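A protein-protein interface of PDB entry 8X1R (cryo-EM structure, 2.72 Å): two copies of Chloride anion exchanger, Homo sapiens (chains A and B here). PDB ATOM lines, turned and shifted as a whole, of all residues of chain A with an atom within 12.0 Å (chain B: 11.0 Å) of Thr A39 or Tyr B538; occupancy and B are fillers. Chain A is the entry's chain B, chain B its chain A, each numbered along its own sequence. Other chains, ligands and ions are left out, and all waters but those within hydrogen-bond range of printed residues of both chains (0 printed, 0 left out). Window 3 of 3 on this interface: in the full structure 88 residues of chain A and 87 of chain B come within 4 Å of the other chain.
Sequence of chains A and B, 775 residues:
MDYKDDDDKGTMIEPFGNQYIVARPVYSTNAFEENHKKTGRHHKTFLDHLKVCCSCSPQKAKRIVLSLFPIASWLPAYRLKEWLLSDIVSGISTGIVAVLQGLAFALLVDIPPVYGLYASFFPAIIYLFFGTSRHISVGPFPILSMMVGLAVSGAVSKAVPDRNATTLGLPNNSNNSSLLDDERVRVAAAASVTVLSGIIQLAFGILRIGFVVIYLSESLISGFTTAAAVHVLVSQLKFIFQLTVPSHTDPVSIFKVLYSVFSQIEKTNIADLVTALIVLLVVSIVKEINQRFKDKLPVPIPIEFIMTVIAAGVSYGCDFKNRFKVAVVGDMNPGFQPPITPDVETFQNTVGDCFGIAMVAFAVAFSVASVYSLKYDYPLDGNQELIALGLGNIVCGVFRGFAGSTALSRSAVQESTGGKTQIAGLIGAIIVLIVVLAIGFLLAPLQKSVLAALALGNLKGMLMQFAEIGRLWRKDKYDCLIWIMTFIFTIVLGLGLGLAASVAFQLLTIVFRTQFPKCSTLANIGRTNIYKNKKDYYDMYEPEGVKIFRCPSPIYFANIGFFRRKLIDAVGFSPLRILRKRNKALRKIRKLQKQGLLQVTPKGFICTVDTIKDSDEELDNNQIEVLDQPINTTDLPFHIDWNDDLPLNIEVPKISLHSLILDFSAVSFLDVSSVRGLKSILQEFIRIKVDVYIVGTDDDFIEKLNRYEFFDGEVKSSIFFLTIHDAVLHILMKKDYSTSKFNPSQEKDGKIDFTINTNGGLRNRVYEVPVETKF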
ATOM      1  N   TYR A  27      30.428  -3.665  12.503  1.00  0.00           N
ATOM      2  CA  TYR A  27      30.440  -4.943  11.806  1.00  0.00           C
ATOM      3  C   TYR A  27      31.866  -5.431  11.628  1.00  0.00           C
ATOM      4  O   TYR A  27      32.690  -4.743  11.021  1.00  0.00           O
ATOM      5  CB  TYR A  27      29.758  -4.827  10.443  1.00  0.00           C
ATOM      6  CG  TYR A  27      28.271  -5.065  10.471  1.00  0.00           C
ATOM      7  CD1 TYR A  27      27.740  -6.161  11.125  1.00  0.00           C
ATOM      8  CD2 TYR A  27      27.400  -4.193   9.843  1.00  0.00           C
ATOM      9  CE1 TYR A  27      26.389  -6.382  11.155  1.00  0.00           C
ATOM     10  CE2 TYR A  27      26.045  -4.406   9.868  1.00  0.00           C
ATOM     11  CZ  TYR A  27      25.545  -5.503  10.524  1.00  0.00           C
ATOM     12  OH  TYR A  27      24.190  -5.726  10.554  1.00  0.00           O
ATOM     13  N   PHE A  32      29.170  -9.501   9.983  1.00  0.00           N
ATOM     14  CA  PHE A  32      28.423  -9.144   8.785  1.00  0.00           C
ATOM     15  C   PHE A  32      27.925 -10.380   8.050  1.00  0.00           C
ATOM     16  O   PHE A  32      26.724 -10.502   7.789  1.00  0.00           O
ATOM     17  CB  PHE A  32      29.287  -8.290   7.861  1.00  0.00           C
ATOM     18  CG  PHE A  32      28.546  -7.734   6.689  1.00  0.00           C
ATOM     19  CD1 PHE A  32      27.584  -6.762   6.865  1.00  0.00           C
ATOM     20  CD2 PHE A  32      28.798  -8.190   5.414  1.00  0.00           C
ATOM     21  CE1 PHE A  32      26.898  -6.253   5.796  1.00  0.00           C
ATOM     22  CE2 PHE A  32      28.113  -7.682   4.343  1.00  0.00           C
ATOM     23  CZ  PHE A  32      27.163  -6.711   4.537  1.00  0.00           C
ATOM     24  N   GLU A  33      28.824 -11.308   7.716  1.00  0.00           N
ATOM     25  CA  GLU A  33      28.408 -12.526   7.029  1.00  0.00           C
ATOM     26  C   GLU A  33      27.449 -13.355   7.873  1.00  0.00           C
ATOM     27  O   GLU A  33      26.678 -14.152   7.327  1.00  0.00           O
ATOM     28  CB  GLU A  33      29.631 -13.358   6.649  1.00  0.00           C
ATOM     29  CG  GLU A  33      30.601 -12.649   5.721  1.00  0.00           C
ATOM     30  CD  GLU A  33      31.959 -13.324   5.677  1.00  0.00           C
ATOM     31  OE1 GLU A  33      32.845 -12.839   4.941  1.00  0.00           O
ATOM     32  OE2 GLU A  33      32.143 -14.339   6.384  1.00  0.00           O
ATOM     33  N   GLU A  34      27.483 -13.191   9.194  1.00  0.00           N
ATOM     34  CA  GLU A  34      26.549 -13.908  10.052  1.00  0.00           C
ATOM     35  C   GLU A  34      25.152 -13.309   9.979  1.00  0.00           C
ATOM     36  O   GLU A  34      24.164 -14.041   9.846  1.00  0.00           O
ATOM     37  CB  GLU A  34      27.060 -13.901  11.490  1.00  0.00           C
ATOM     38  CG  GLU A  34      26.155 -14.604  12.474  1.00  0.00           C
ATOM     39  CD  GLU A  34      26.308 -14.062  13.878  1.00  0.00           C
ATOM     40  OE1 GLU A  34      27.454 -13.778  14.281  1.00  0.00           O
ATOM     41  OE2 GLU A  34      25.282 -13.918  14.577  1.00  0.00           O
ATOM     42  N   ASN A  35      25.042 -11.983  10.070  1.00  0.00           N
ATOM     43  CA  ASN A  35      23.720 -11.364  10.071  1.00  0.00           C
ATOM     44  C   ASN A  35      23.108 -11.317   8.676  1.00  0.00           C
ATOM     45  O   ASN A  35      21.887 -11.428   8.530  1.00  0.00           O
ATOM     46  CB  ASN A  35      23.794  -9.962  10.667  1.00  0.00           C
ATOM     47  CG  ASN A  35      24.057  -9.979  12.155  1.00  0.00           C
ATOM     48  OD1 ASN A  35      25.203 -10.016  12.595  1.00  0.00           O
ATOM     49  ND2 ASN A  35      22.989  -9.959  12.941  1.00  0.00           N
ATOM     50  N   HIS A  36      23.928 -11.151   7.646  1.00  0.00           N
ATOM     51  CA  HIS A  36      23.452 -11.117   6.271  1.00  0.00           C
ATOM     52  C   HIS A  36      23.817 -12.412   5.568  1.00  0.00           C
ATOM     53  O   HIS A  36      24.965 -12.605   5.161  1.00  0.00           O
ATOM     54  CB  HIS A  36      24.049  -9.932   5.513  1.00  0.00           C
ATOM     55  CG  HIS A  36      23.672  -8.602   6.083  1.00  0.00           C
ATOM     56  ND1 HIS A  36      24.480  -7.914   6.959  1.00  0.00           N
ATOM     57  CD2 HIS A  36      22.570  -7.838   5.905  1.00  0.00           C
ATOM     58  CE1 HIS A  36      23.895  -6.780   7.294  1.00  0.00           C
ATOM     59  NE2 HIS A  36      22.734  -6.709   6.670  1.00  0.00           N
ATOM     60  N   LYS A  37      22.832 -13.296   5.419  1.00  0.00           N
ATOM     61  CA  LYS A  37      23.083 -14.580   4.787  1.00  0.00           C
ATOM     62  C   LYS A  37      23.530 -14.379   3.339  1.00  0.00           C
ATOM     63  O   LYS A  37      23.014 -13.540   2.602  1.00  0.00           O
ATOM     64  CB  LYS A  37      21.853 -15.491   4.864  1.00  0.00           C
ATOM     65  N   LYS A  38      24.504 -15.192   2.939  1.00  0.00           N
ATOM     66  CA  LYS A  38      25.282 -14.968   1.724  1.00  0.00           C
ATOM     67  C   LYS A  38      24.866 -15.997   0.685  1.00  0.00           C
ATOM     68  O   LYS A  38      24.782 -17.189   0.991  1.00  0.00           O
ATOM     69  CB  LYS A  38      26.777 -15.061   2.029  1.00  0.00           C
ATOM     70  CG  LYS A  38      27.694 -14.854   0.847  1.00  0.00           C
ATOM     71  CD  LYS A  38      29.102 -14.542   1.318  1.00  0.00           C
ATOM     72  CE  LYS A  38      30.007 -14.178   0.160  1.00  0.00           C
ATOM     73  NZ  LYS A  38      31.417 -14.017   0.601  1.00  0.00           N
ATOM     74  N   THR A  39      24.597 -15.539  -0.533  1.00  0.00           N
ATOM     75  CA  THR A  39      24.207 -16.431  -1.617  1.00  0.00           C
ATOM     76  C   THR A  39      25.323 -17.414  -1.931  1.00  0.00           C
ATOM     77  O   THR A  39      26.431 -17.016  -2.304  1.00  0.00           O
ATOM     78  CB  THR A  39      23.851 -15.617  -2.865  1.00  0.00           C
ATOM     79  OG1 THR A  39      22.544 -15.051  -2.717  1.00  0.00           O
ATOM     80  CG2 THR A  39      23.875 -16.492  -4.098  1.00  0.00           C
ATOM     81  N   GLY A  40      25.032 -18.703  -1.775  1.00  0.00           N
ATOM     82  CA  GLY A  40      26.033 -19.710  -2.075  1.00  0.00           C
ATOM     83  C   GLY A  40      26.212 -19.871  -3.574  1.00  0.00           C
ATOM     84  O   GLY A  40      25.266 -20.166  -4.306  1.00  0.00           O
ATOM     85  N   ARG A  41      27.446 -19.671  -4.032  1.00  0.00           N
ATOM     86  CA  ARG A  41      27.758 -19.729  -5.454  1.00  0.00           C
ATOM     87  C   ARG A  41      28.823 -20.784  -5.690  1.00  0.00           C
ATOM     88  O   ARG A  41      29.892 -20.739  -5.073  1.00  0.00           O
ATOM     89  CB  ARG A  41      28.241 -18.373  -5.981  1.00  0.00           C
ATOM     90  CG  ARG A  41      27.565 -17.166  -5.365  1.00  0.00           C
ATOM     91  CD  ARG A  41      28.521 -15.987  -5.298  1.00  0.00           C
ATOM     92  NE  ARG A  41      29.085 -15.662  -6.606  1.00  0.00           N
ATOM     93  CZ  ARG A  41      30.107 -14.832  -6.792  1.00  0.00           C
ATOM     94  NH1 ARG A  41      30.676 -14.236  -5.754  1.00  0.00           N
ATOM     95  NH2 ARG A  41      30.559 -14.593  -8.014  1.00  0.00           N
ATOM     96  N   HIS A  42      28.529 -21.729  -6.581  1.00  0.00           N
ATOM     97  CA  HIS A  42      29.538 -22.636  -7.106  1.00  0.00           C
ATOM     98  C   HIS A  42      30.432 -21.963  -8.136  1.00  0.00           C
ATOM     99  O   HIS A  42      30.136 -22.064  -9.332  1.00  0.00           O
ATOM    100  CB  HIS A  42      28.863 -23.865  -7.724  1.00  0.00           C
ATOM    101  CG  HIS A  42      29.820 -24.936  -8.144  1.00  0.00           C
ATOM    102  ND1 HIS A  42      30.515 -24.891  -9.334  1.00  0.00           N
ATOM    103  CD2 HIS A  42      30.199 -26.082  -7.530  1.00  0.00           C
ATOM    104  CE1 HIS A  42      31.280 -25.964  -9.437  1.00  0.00           C
ATOM    105  NE2 HIS A  42      31.107 -26.703  -8.355  1.00  0.00           N
ATOM    106  N   HIS A  43      31.487 -21.266  -7.701  1.00  0.00           N
ATOM    107  CA  HIS A  43      32.247 -20.316  -8.530  1.00  0.00           C
ATOM    108  C   HIS A  43      32.594 -20.989  -9.859  1.00  0.00           C
ATOM    109  O   HIS A  43      32.037 -20.579 -10.885  1.00  0.00           O
ATOM    110  CB  HIS A  43      33.435 -19.816  -7.721  1.00  0.00           C
ATOM    111  CG  HIS A  43      34.271 -18.799  -8.437  1.00  0.00           C
ATOM    112  ND1 HIS A  43      33.774 -17.578  -8.834  1.00  0.00           N
ATOM    113  CD2 HIS A  43      35.567 -18.822  -8.825  1.00  0.00           C
ATOM    114  CE1 HIS A  43      34.728 -16.890  -9.436  1.00  0.00           C
ATOM    115  NE2 HIS A  43      35.827 -17.623  -9.444  1.00  0.00           N
ATOM    116  N   LYS A  44      33.317 -22.129  -9.833  1.00  0.00           N
ATOM    117  CA  LYS A  44      33.753 -22.944 -10.991  1.00  0.00           C
ATOM    118  C   LYS A  44      34.687 -23.997 -10.513  1.00  0.00           C
ATOM    119  O   LYS A  44      35.257 -23.930  -9.423  1.00  0.00           O
ATOM    120  CB  LYS A  44      34.440 -22.176 -12.158  1.00  0.00           C
ATOM    121  CG  LYS A  44      33.550 -21.949 -13.371  1.00  0.00           C
ATOM    122  CD  LYS A  44      33.031 -23.265 -13.924  1.00  0.00           C
ATOM    123  CE  LYS A  44      32.117 -23.043 -15.119  1.00  0.00           C
ATOM    124  NZ  LYS A  44      31.596 -24.328 -15.663  1.00  0.00           N
ATOM    125  N   ASP A 699      35.600  -9.695   0.219  1.00  0.00           N
ATOM    126  CA  ASP A 699      35.431 -11.080   0.644  1.00  0.00           C
ATOM    127  C   ASP A 699      36.358 -12.028  -0.104  1.00  0.00           C
ATOM    128  O   ASP A 699      36.766 -13.056   0.450  1.00  0.00           O
ATOM    129  CB  ASP A 699      33.978 -11.510   0.460  1.00  0.00           C
ATOM    130  CG  ASP A 699      33.007 -10.614   1.205  1.00  0.00           C
ATOM    131  OD1 ASP A 699      31.872 -10.432   0.718  1.00  0.00           O
ATOM    132  OD2 ASP A 699      33.380 -10.088   2.275  1.00  0.00           O
ATOM    133  N   ASP A 700      36.705 -11.703  -1.349  1.00  0.00           N
ATOM    134  CA  ASP A 700      37.643 -12.535  -2.093  1.00  0.00           C
ATOM    135  C   ASP A 700      39.022 -12.526  -1.451  1.00  0.00           C
ATOM    136  O   ASP A 700      39.727 -13.539  -1.481  1.00  0.00           O
ATOM    137  CB  ASP A 700      37.727 -12.063  -3.542  1.00  0.00           C
ATOM    138  CG  ASP A 700      36.382 -12.083  -4.239  1.00  0.00           C
ATOM    139  OD1 ASP A 700      35.564 -11.173  -3.987  1.00  0.00           O
ATOM    140  OD2 ASP A 700      36.141 -13.008  -5.042  1.00  0.00           O
ATOM    141  N   GLU A 703      38.815 -14.915   1.448  1.00  0.00           N
ATOM    142  CA  GLU A 703      38.704 -16.279   0.944  1.00  0.00           C
ATOM    143  C   GLU A 703      40.045 -16.779   0.424  1.00  0.00           C
ATOM    144  O   GLU A 703      40.384 -17.956   0.589  1.00  0.00           O
ATOM    145  CB  GLU A 703      37.640 -16.355  -0.147  1.00  0.00           C
ATOM    146  CG  GLU A 703      37.413 -17.761  -0.674  1.00  0.00           C
ATOM    147  CD  GLU A 703      36.848 -18.699   0.368  1.00  0.00           C
ATOM    148  OE1 GLU A 703      36.398 -18.213   1.428  1.00  0.00           O
ATOM    149  OE2 GLU A 703      36.844 -19.924   0.125  1.00  0.00           O
ATOM    150  N   ALA B 523      26.449  -3.468  -4.854  1.00  0.00           N
ATOM    151  CA  ALA B 523      25.090  -3.118  -4.484  1.00  0.00           C
ATOM    152  C   ALA B 523      25.024  -2.959  -2.972  1.00  0.00           C
ATOM    153  O   ALA B 523      25.907  -3.411  -2.239  1.00  0.00           O
ATOM    154  CB  ALA B 523      24.085  -4.165  -4.966  1.00  0.00           C
ATOM    155  N   ASN B 524      23.950  -2.321  -2.520  1.00  0.00           N
ATOM    156  CA  ASN B 524      23.789  -1.933  -1.128  1.00  0.00           C
ATOM    157  C   ASN B 524      23.086  -3.022  -0.324  1.00  0.00           C
ATOM    158  O   ASN B 524      22.091  -3.600  -0.762  1.00  0.00           O
ATOM    159  CB  ASN B 524      22.989  -0.635  -1.051  1.00  0.00           C
ATOM    160  CG  ASN B 524      23.151   0.073   0.263  1.00  0.00           C
ATOM    161  OD1 ASN B 524      24.007  -0.276   1.065  1.00  0.00           O
ATOM    162  ND2 ASN B 524      22.327   1.082   0.492  1.00  0.00           N
ATOM    163  N   ILE B 525      23.608  -3.288   0.872  1.00  0.00           N
ATOM    164  CA  ILE B 525      23.022  -4.259   1.792  1.00  0.00           C
ATOM    165  C   ILE B 525      22.679  -3.545   3.088  1.00  0.00           C
ATOM    166  O   ILE B 525      23.557  -2.951   3.723  1.00  0.00           O
ATOM    167  CB  ILE B 525      23.964  -5.434   2.083  1.00  0.00           C
ATOM    168  CG1 ILE B 525      24.188  -6.259   0.831  1.00  0.00           C
ATOM    169  CG2 ILE B 525      23.385  -6.321   3.170  1.00  0.00           C
ATOM    170  CD1 ILE B 525      25.281  -7.241   0.987  1.00  0.00           C
ATOM    171  N   GLY B 526      21.415  -3.616   3.487  1.00  0.00           N
ATOM    172  CA  GLY B 526      20.991  -3.099   4.769  1.00  0.00           C
ATOM    173  C   GLY B 526      20.553  -1.656   4.783  1.00  0.00           C
ATOM    174  O   GLY B 526      20.261  -1.133   5.864  1.00  0.00           O
ATOM    175  N   ARG B 527      20.496  -0.997   3.626  1.00  0.00           N
ATOM    176  CA  ARG B 527      20.111   0.411   3.536  1.00  0.00           C
ATOM    177  C   ARG B 527      21.047   1.290   4.361  1.00  0.00           C
ATOM    178  O   ARG B 527      20.616   2.186   5.087  1.00  0.00           O
ATOM    179  CB  ARG B 527      18.656   0.614   3.955  1.00  0.00           C
ATOM    180  CG  ARG B 527      17.656  -0.085   3.053  1.00  0.00           C
ATOM    181  CD  ARG B 527      17.568   0.599   1.702  1.00  0.00           C
ATOM    182  NE  ARG B 527      16.634  -0.077   0.810  1.00  0.00           N
ATOM    183  CZ  ARG B 527      15.871   0.546  -0.081  1.00  0.00           C
ATOM    184  NH1 ARG B 527      15.929   1.865  -0.196  1.00  0.00           N
ATOM    185  NH2 ARG B 527      15.048  -0.149  -0.853  1.00  0.00           N
ATOM    186  N   ILE B 530      27.164   0.222   3.252  1.00  0.00           N
ATOM    187  CA  ILE B 530      27.911  -0.989   2.930  1.00  0.00           C
ATOM    188  C   ILE B 530      27.535  -1.420   1.521  1.00  0.00           C
ATOM    189  O   ILE B 530      26.359  -1.662   1.235  1.00  0.00           O
ATOM    190  CB  ILE B 530      27.636  -2.115   3.935  1.00  0.00           C
ATOM    191  CG1 ILE B 530      27.775  -1.607   5.364  1.00  0.00           C
ATOM    192  CG2 ILE B 530      28.574  -3.280   3.695  1.00  0.00           C
ATOM    193  CD1 ILE B 530      27.311  -2.589   6.391  1.00  0.00           C
ATOM    194  N   LYS B 532      28.597  -4.244  -1.394  1.00  0.00           N
ATOM    195  CA  LYS B 532      29.308  -5.491  -1.643  1.00  0.00           C
ATOM    196  C   LYS B 532      28.867  -6.081  -2.976  1.00  0.00           C
ATOM    197  O   LYS B 532      27.959  -5.574  -3.628  1.00  0.00           O
ATOM    198  CB  LYS B 532      29.086  -6.487  -0.503  1.00  0.00           C
ATOM    199  CG  LYS B 532      29.475  -5.960   0.863  1.00  0.00           C
ATOM    200  CD  LYS B 532      30.436  -6.881   1.568  1.00  0.00           C
ATOM    201  CE  LYS B 532      31.256  -6.124   2.583  1.00  0.00           C
ATOM    202  NZ  LYS B 532      32.284  -5.272   1.929  1.00  0.00           N
ATOM    203  N   ASN B 533      29.521  -7.173  -3.364  1.00  0.00           N
ATOM    204  CA  ASN B 533      29.294  -7.787  -4.666  1.00  0.00           C
ATOM    205  C   ASN B 533      27.816  -8.068  -4.896  1.00  0.00           C
ATOM    206  O   ASN B 533      27.151  -8.682  -4.062  1.00  0.00           O
ATOM    207  CB  ASN B 533      30.093  -9.081  -4.774  1.00  0.00           C
ATOM    208  CG  ASN B 533      30.390  -9.463  -6.201  1.00  0.00           C
ATOM    209  OD1 ASN B 533      29.593  -9.221  -7.099  1.00  0.00           O
ATOM    210  ND2 ASN B 533      31.543 -10.072  -6.418  1.00  0.00           N
ATOM    211  N   LYS B 534      27.313  -7.626  -6.049  1.00  0.00           N
ATOM    212  CA  LYS B 534      25.897  -7.752  -6.370  1.00  0.00           C
ATOM    213  C   LYS B 534      25.442  -9.203  -6.434  1.00  0.00           C
ATOM    214  O   LYS B 534      24.244  -9.474  -6.300  1.00  0.00           O
ATOM    215  CB  LYS B 534      25.626  -7.055  -7.701  1.00  0.00           C
ATOM    216  CG  LYS B 534      24.183  -6.920  -8.096  1.00  0.00           C
ATOM    217  CD  LYS B 534      24.089  -6.573  -9.568  1.00  0.00           C
ATOM    218  CE  LYS B 534      22.676  -6.719 -10.087  1.00  0.00           C
ATOM    219  NZ  LYS B 534      22.586  -6.343 -11.522  1.00  0.00           N
ATOM    220  N   LYS B 535      26.367 -10.138  -6.622  1.00  0.00           N
ATOM    221  CA  LYS B 535      26.046 -11.546  -6.785  1.00  0.00           C
ATOM    222  C   LYS B 535      26.277 -12.365  -5.526  1.00  0.00           C
ATOM    223  O   LYS B 535      26.203 -13.594  -5.587  1.00  0.00           O
ATOM    224  CB  LYS B 535      26.877 -12.136  -7.925  1.00  0.00           C
ATOM    225  CG  LYS B 535      26.648 -11.477  -9.263  1.00  0.00           C
ATOM    226  CD  LYS B 535      27.132 -12.360 -10.392  1.00  0.00           C
ATOM    227  CE  LYS B 535      28.593 -12.716 -10.215  1.00  0.00           C
ATOM    228  NZ  LYS B 535      29.170 -13.274 -11.464  1.00  0.00           N
ATOM    229  N   ASP B 536      26.545 -11.726  -4.391  1.00  0.00           N
ATOM    230  CA  ASP B 536      27.013 -12.443  -3.214  1.00  0.00           C
ATOM    231  C   ASP B 536      25.970 -12.591  -2.120  1.00  0.00           C
ATOM    232  O   ASP B 536      25.994 -13.594  -1.404  1.00  0.00           O
ATOM    233  CB  ASP B 536      28.244 -11.748  -2.632  1.00  0.00           C
ATOM    234  CG  ASP B 536      29.531 -12.240  -3.246  1.00  0.00           C
ATOM    235  OD1 ASP B 536      29.467 -13.007  -4.224  1.00  0.00           O
ATOM    236  OD2 ASP B 536      30.611 -11.863  -2.751  1.00  0.00           O
ATOM    237  N   TYR B 537      25.057 -11.641  -1.958  1.00  0.00           N
ATOM    238  CA  TYR B 537      24.115 -11.679  -0.851  1.00  0.00           C
ATOM    239  C   TYR B 537      22.691 -11.575  -1.374  1.00  0.00           C
ATOM    240  O   TYR B 537      22.455 -11.254  -2.539  1.00  0.00           O
ATOM    241  CB  TYR B 537      24.378 -10.554   0.162  1.00  0.00           C
ATOM    242  CG  TYR B 537      25.782 -10.541   0.721  1.00  0.00           C
ATOM    243  CD1 TYR B 537      26.053 -11.063   1.974  1.00  0.00           C
ATOM    244  CD2 TYR B 537      26.833 -10.001  -0.001  1.00  0.00           C
ATOM    245  CE1 TYR B 537      27.330 -11.056   2.484  1.00  0.00           C
ATOM    246  CE2 TYR B 537      28.110  -9.992   0.500  1.00  0.00           C
ATOM    247  CZ  TYR B 537      28.353 -10.518   1.743  1.00  0.00           C
ATOM    248  OH  TYR B 537      29.630 -10.507   2.246  1.00  0.00           O
ATOM    249  N   TYR B 538      21.742 -11.863  -0.491  1.00  0.00           N
ATOM    250  CA  TYR B 538      20.333 -11.686  -0.790  1.00  0.00           C
ATOM    251  C   TYR B 538      19.859 -10.319  -0.312  1.00  0.00           C
ATOM    252  O   TYR B 538      20.479  -9.681   0.544  1.00  0.00           O
ATOM    253  CB  TYR B 538      19.492 -12.774  -0.123  1.00  0.00           C
ATOM    254  CG  TYR B 538      19.647 -14.154  -0.716  1.00  0.00           C
ATOM    255  CD1 TYR B 538      19.267 -14.417  -2.025  1.00  0.00           C
ATOM    256  CD2 TYR B 538      20.155 -15.200   0.040  1.00  0.00           C
ATOM    257  CE1 TYR B 538      19.401 -15.677  -2.565  1.00  0.00           C
ATOM    258  CE2 TYR B 538      20.293 -16.462  -0.493  1.00  0.00           C
ATOM    259  CZ  TYR B 538      19.914 -16.695  -1.795  1.00  0.00           C
ATOM    260  OH  TYR B 538      20.050 -17.955  -2.328  1.00  0.00           O
ATOM    261  N   ASP B 539      18.741  -9.871  -0.882  1.00  0.00           N
ATOM    262  CA  ASP B 539      18.063  -8.650  -0.451  1.00  0.00           C
ATOM    263  C   ASP B 539      18.929  -7.409  -0.644  1.00  0.00           C
ATOM    264  O   ASP B 539      18.841  -6.453   0.129  1.00  0.00           O
ATOM    265  CB  ASP B 539      17.607  -8.755   1.007  1.00  0.00           C
ATOM    266  CG  ASP B 539      16.279  -9.463   1.154  1.00  0.00           C
ATOM    267  OD1 ASP B 539      15.854 -10.141   0.194  1.00  0.00           O
ATOM    268  OD2 ASP B 539      15.659  -9.345   2.230  1.00  0.00           O
ATOM    269  N   MET B 540      19.770  -7.404  -1.671  1.00  0.00           N
ATOM    270  CA  MET B 540      20.557  -6.228  -1.999  1.00  0.00           C
ATOM    271  C   MET B 540      19.714  -5.236  -2.790  1.00  0.00           C
ATOM    272  O   MET B 540      18.576  -5.518  -3.170  1.00  0.00           O
ATOM    273  CB  MET B 540      21.807  -6.618  -2.780  1.00  0.00           C
ATOM    274  CG  MET B 540      22.639  -7.669  -2.083  1.00  0.00           C
ATOM    275  SD  MET B 540      24.106  -8.123  -3.006  1.00  0.00           S
ATOM    276  CE  MET B 540      25.312  -7.121  -2.172  1.00  0.00           C
ATOM    277  N   TYR B 541      20.281  -4.058  -3.034  1.00  0.00           N
ATOM    278  CA  TYR B 541      19.520  -2.948  -3.602  1.00  0.00           C
ATOM    279  C   TYR B 541      20.407  -2.150  -4.546  1.00  0.00           C
ATOM    280  O   TYR B 541      21.473  -1.674  -4.149  1.00  0.00           O
ATOM    281  CB  TYR B 541      18.961  -2.054  -2.497  1.00  0.00           C
ATOM    282  CG  TYR B 541      18.461  -0.715  -2.974  1.00  0.00           C
ATOM    283  CD1 TYR B 541      19.186   0.441  -2.736  1.00  0.00           C
ATOM    284  CD2 TYR B 541      17.258  -0.604  -3.654  1.00  0.00           C
ATOM    285  CE1 TYR B 541      18.732   1.669  -3.167  1.00  0.00           C
ATOM    286  CE2 TYR B 541      16.796   0.620  -4.089  1.00  0.00           C
ATOM    287  CZ  TYR B 541      17.538   1.753  -3.842  1.00  0.00           C
ATOM    288  OH  TYR B 541      17.084   2.976  -4.272  1.00  0.00           O
ATOM    289  N   GLU B 542      19.966  -2.011  -5.794  1.00  0.00           N
ATOM    290  CA  GLU B 542      20.632  -1.166  -6.771  1.00  0.00           C
ATOM    291  C   GLU B 542      19.821   0.104  -6.951  1.00  0.00           C
ATOM    292  O   GLU B 542      18.669   0.020  -7.401  1.00  0.00           O
ATOM    293  CB  GLU B 542      20.763  -1.890  -8.105  1.00  0.00           C
ATOM    294  CG  GLU B 542      21.823  -2.967  -8.157  1.00  0.00           C
ATOM    295  CD  GLU B 542      23.072  -2.513  -8.872  1.00  0.00           C
ATOM    296  OE1 GLU B 542      23.679  -3.333  -9.588  1.00  0.00           O
ATOM    297  OE2 GLU B 542      23.450  -1.334  -8.720  1.00  0.00           O
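The backbone NH of Thr A39 sits at hydrogen-bond distance from the backbone carbonyl oxygen of Asp B536 (2.5 Å). OD1 of Asp B536 lies within salt-bridge range of NE of Arg A41. The side-chain carboxylate of Asp A699 lies within hydrogen-bond range of the side-chain hydroxyl of Tyr B537 (2.7 Å).
The backbone NH of Ala B523 sits at hydrogen-bond distance from the backbone carbonyl oxygen of Lys B532. OD1 of Asn B524 sits close to O of Ile B530 (2.7 Å). The backbone NH (N) of Ile B525 sits at hydrogen-bond distance from the backbone carbonyl oxygen (O) of Ile B530 (3.2 Å). The side-chain amide oxygen of Asn B533 lies close to the backbone NH of Lys B535 (3.4 Å). The side-chain sulfur of Met B540 sits at hydrogen-bond distance from the backbone NH of Tyr B537 (3.8 Å). The side-chain amino group of Lys A38 is in salt-bridge range of the side-chain carboxylate of Asp A699 (3.6 Å).
Phe A32 touches Ile B530 (CE1 to CD1, 3.7 Å). Phe A32 touches Tyr B537. His A36 touches Ile B525. Lys A37 touches Tyr B537 (O to CD1, 3.97 Å). Lys A37 touches Tyr B538. O of Asp B536 touches CG of Lys A38, at 3.1 Å. Lys A38 touches Tyr B537 (CA to CD1, 3.99 Å). Thr A39 touches Tyr B537 (OG1 to C, 3.7 Å). Lys B535 touches Arg A41. OD1 of Asp A699 touches OD2 of Asp B536, 3.96 Å away.
Printed residues of chain B within 4 Å of Thr A39: Asp B536 (2.5 Å), Tyr B537 (3.7 Å) and Tyr B538 (3.2 Å). Tyr B538 touches just these residues of chain A: Lys A37 and Thr A39. Lys A37 touches just these residues of chain B: Tyr B537 and Tyr B538. Gly A40 touches none of the printed residues of chain B. No residue of chain A comes within 4 Å of Asp B539. Met B540 touches none of the printed residues of chain A. Printed residues of chain B within 4 Å of Tyr A27: Ile B530. Of the printed residues of chain B, Phe A32 touches Ile B530 (3.7 Å), Lys B532 (3.7 Å) and Tyr B537 (3.8 Å). Printed residues of chain A within 4 Å of Ile B530: Tyr A27 and Phe A32.
Printed residues of chain A that touch a printed residue of chain B: Tyr A27, Phe A32, His A36, Lys A37, Lys A38, Thr A39, Arg A41 and Asp A699. Among the printed residues, 18 pairs touch across the chains.
No position is printed for both chains. Of the 18 pairs that touch across the chains among the printed residues, none has its exchanged pair printed and touching as well.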
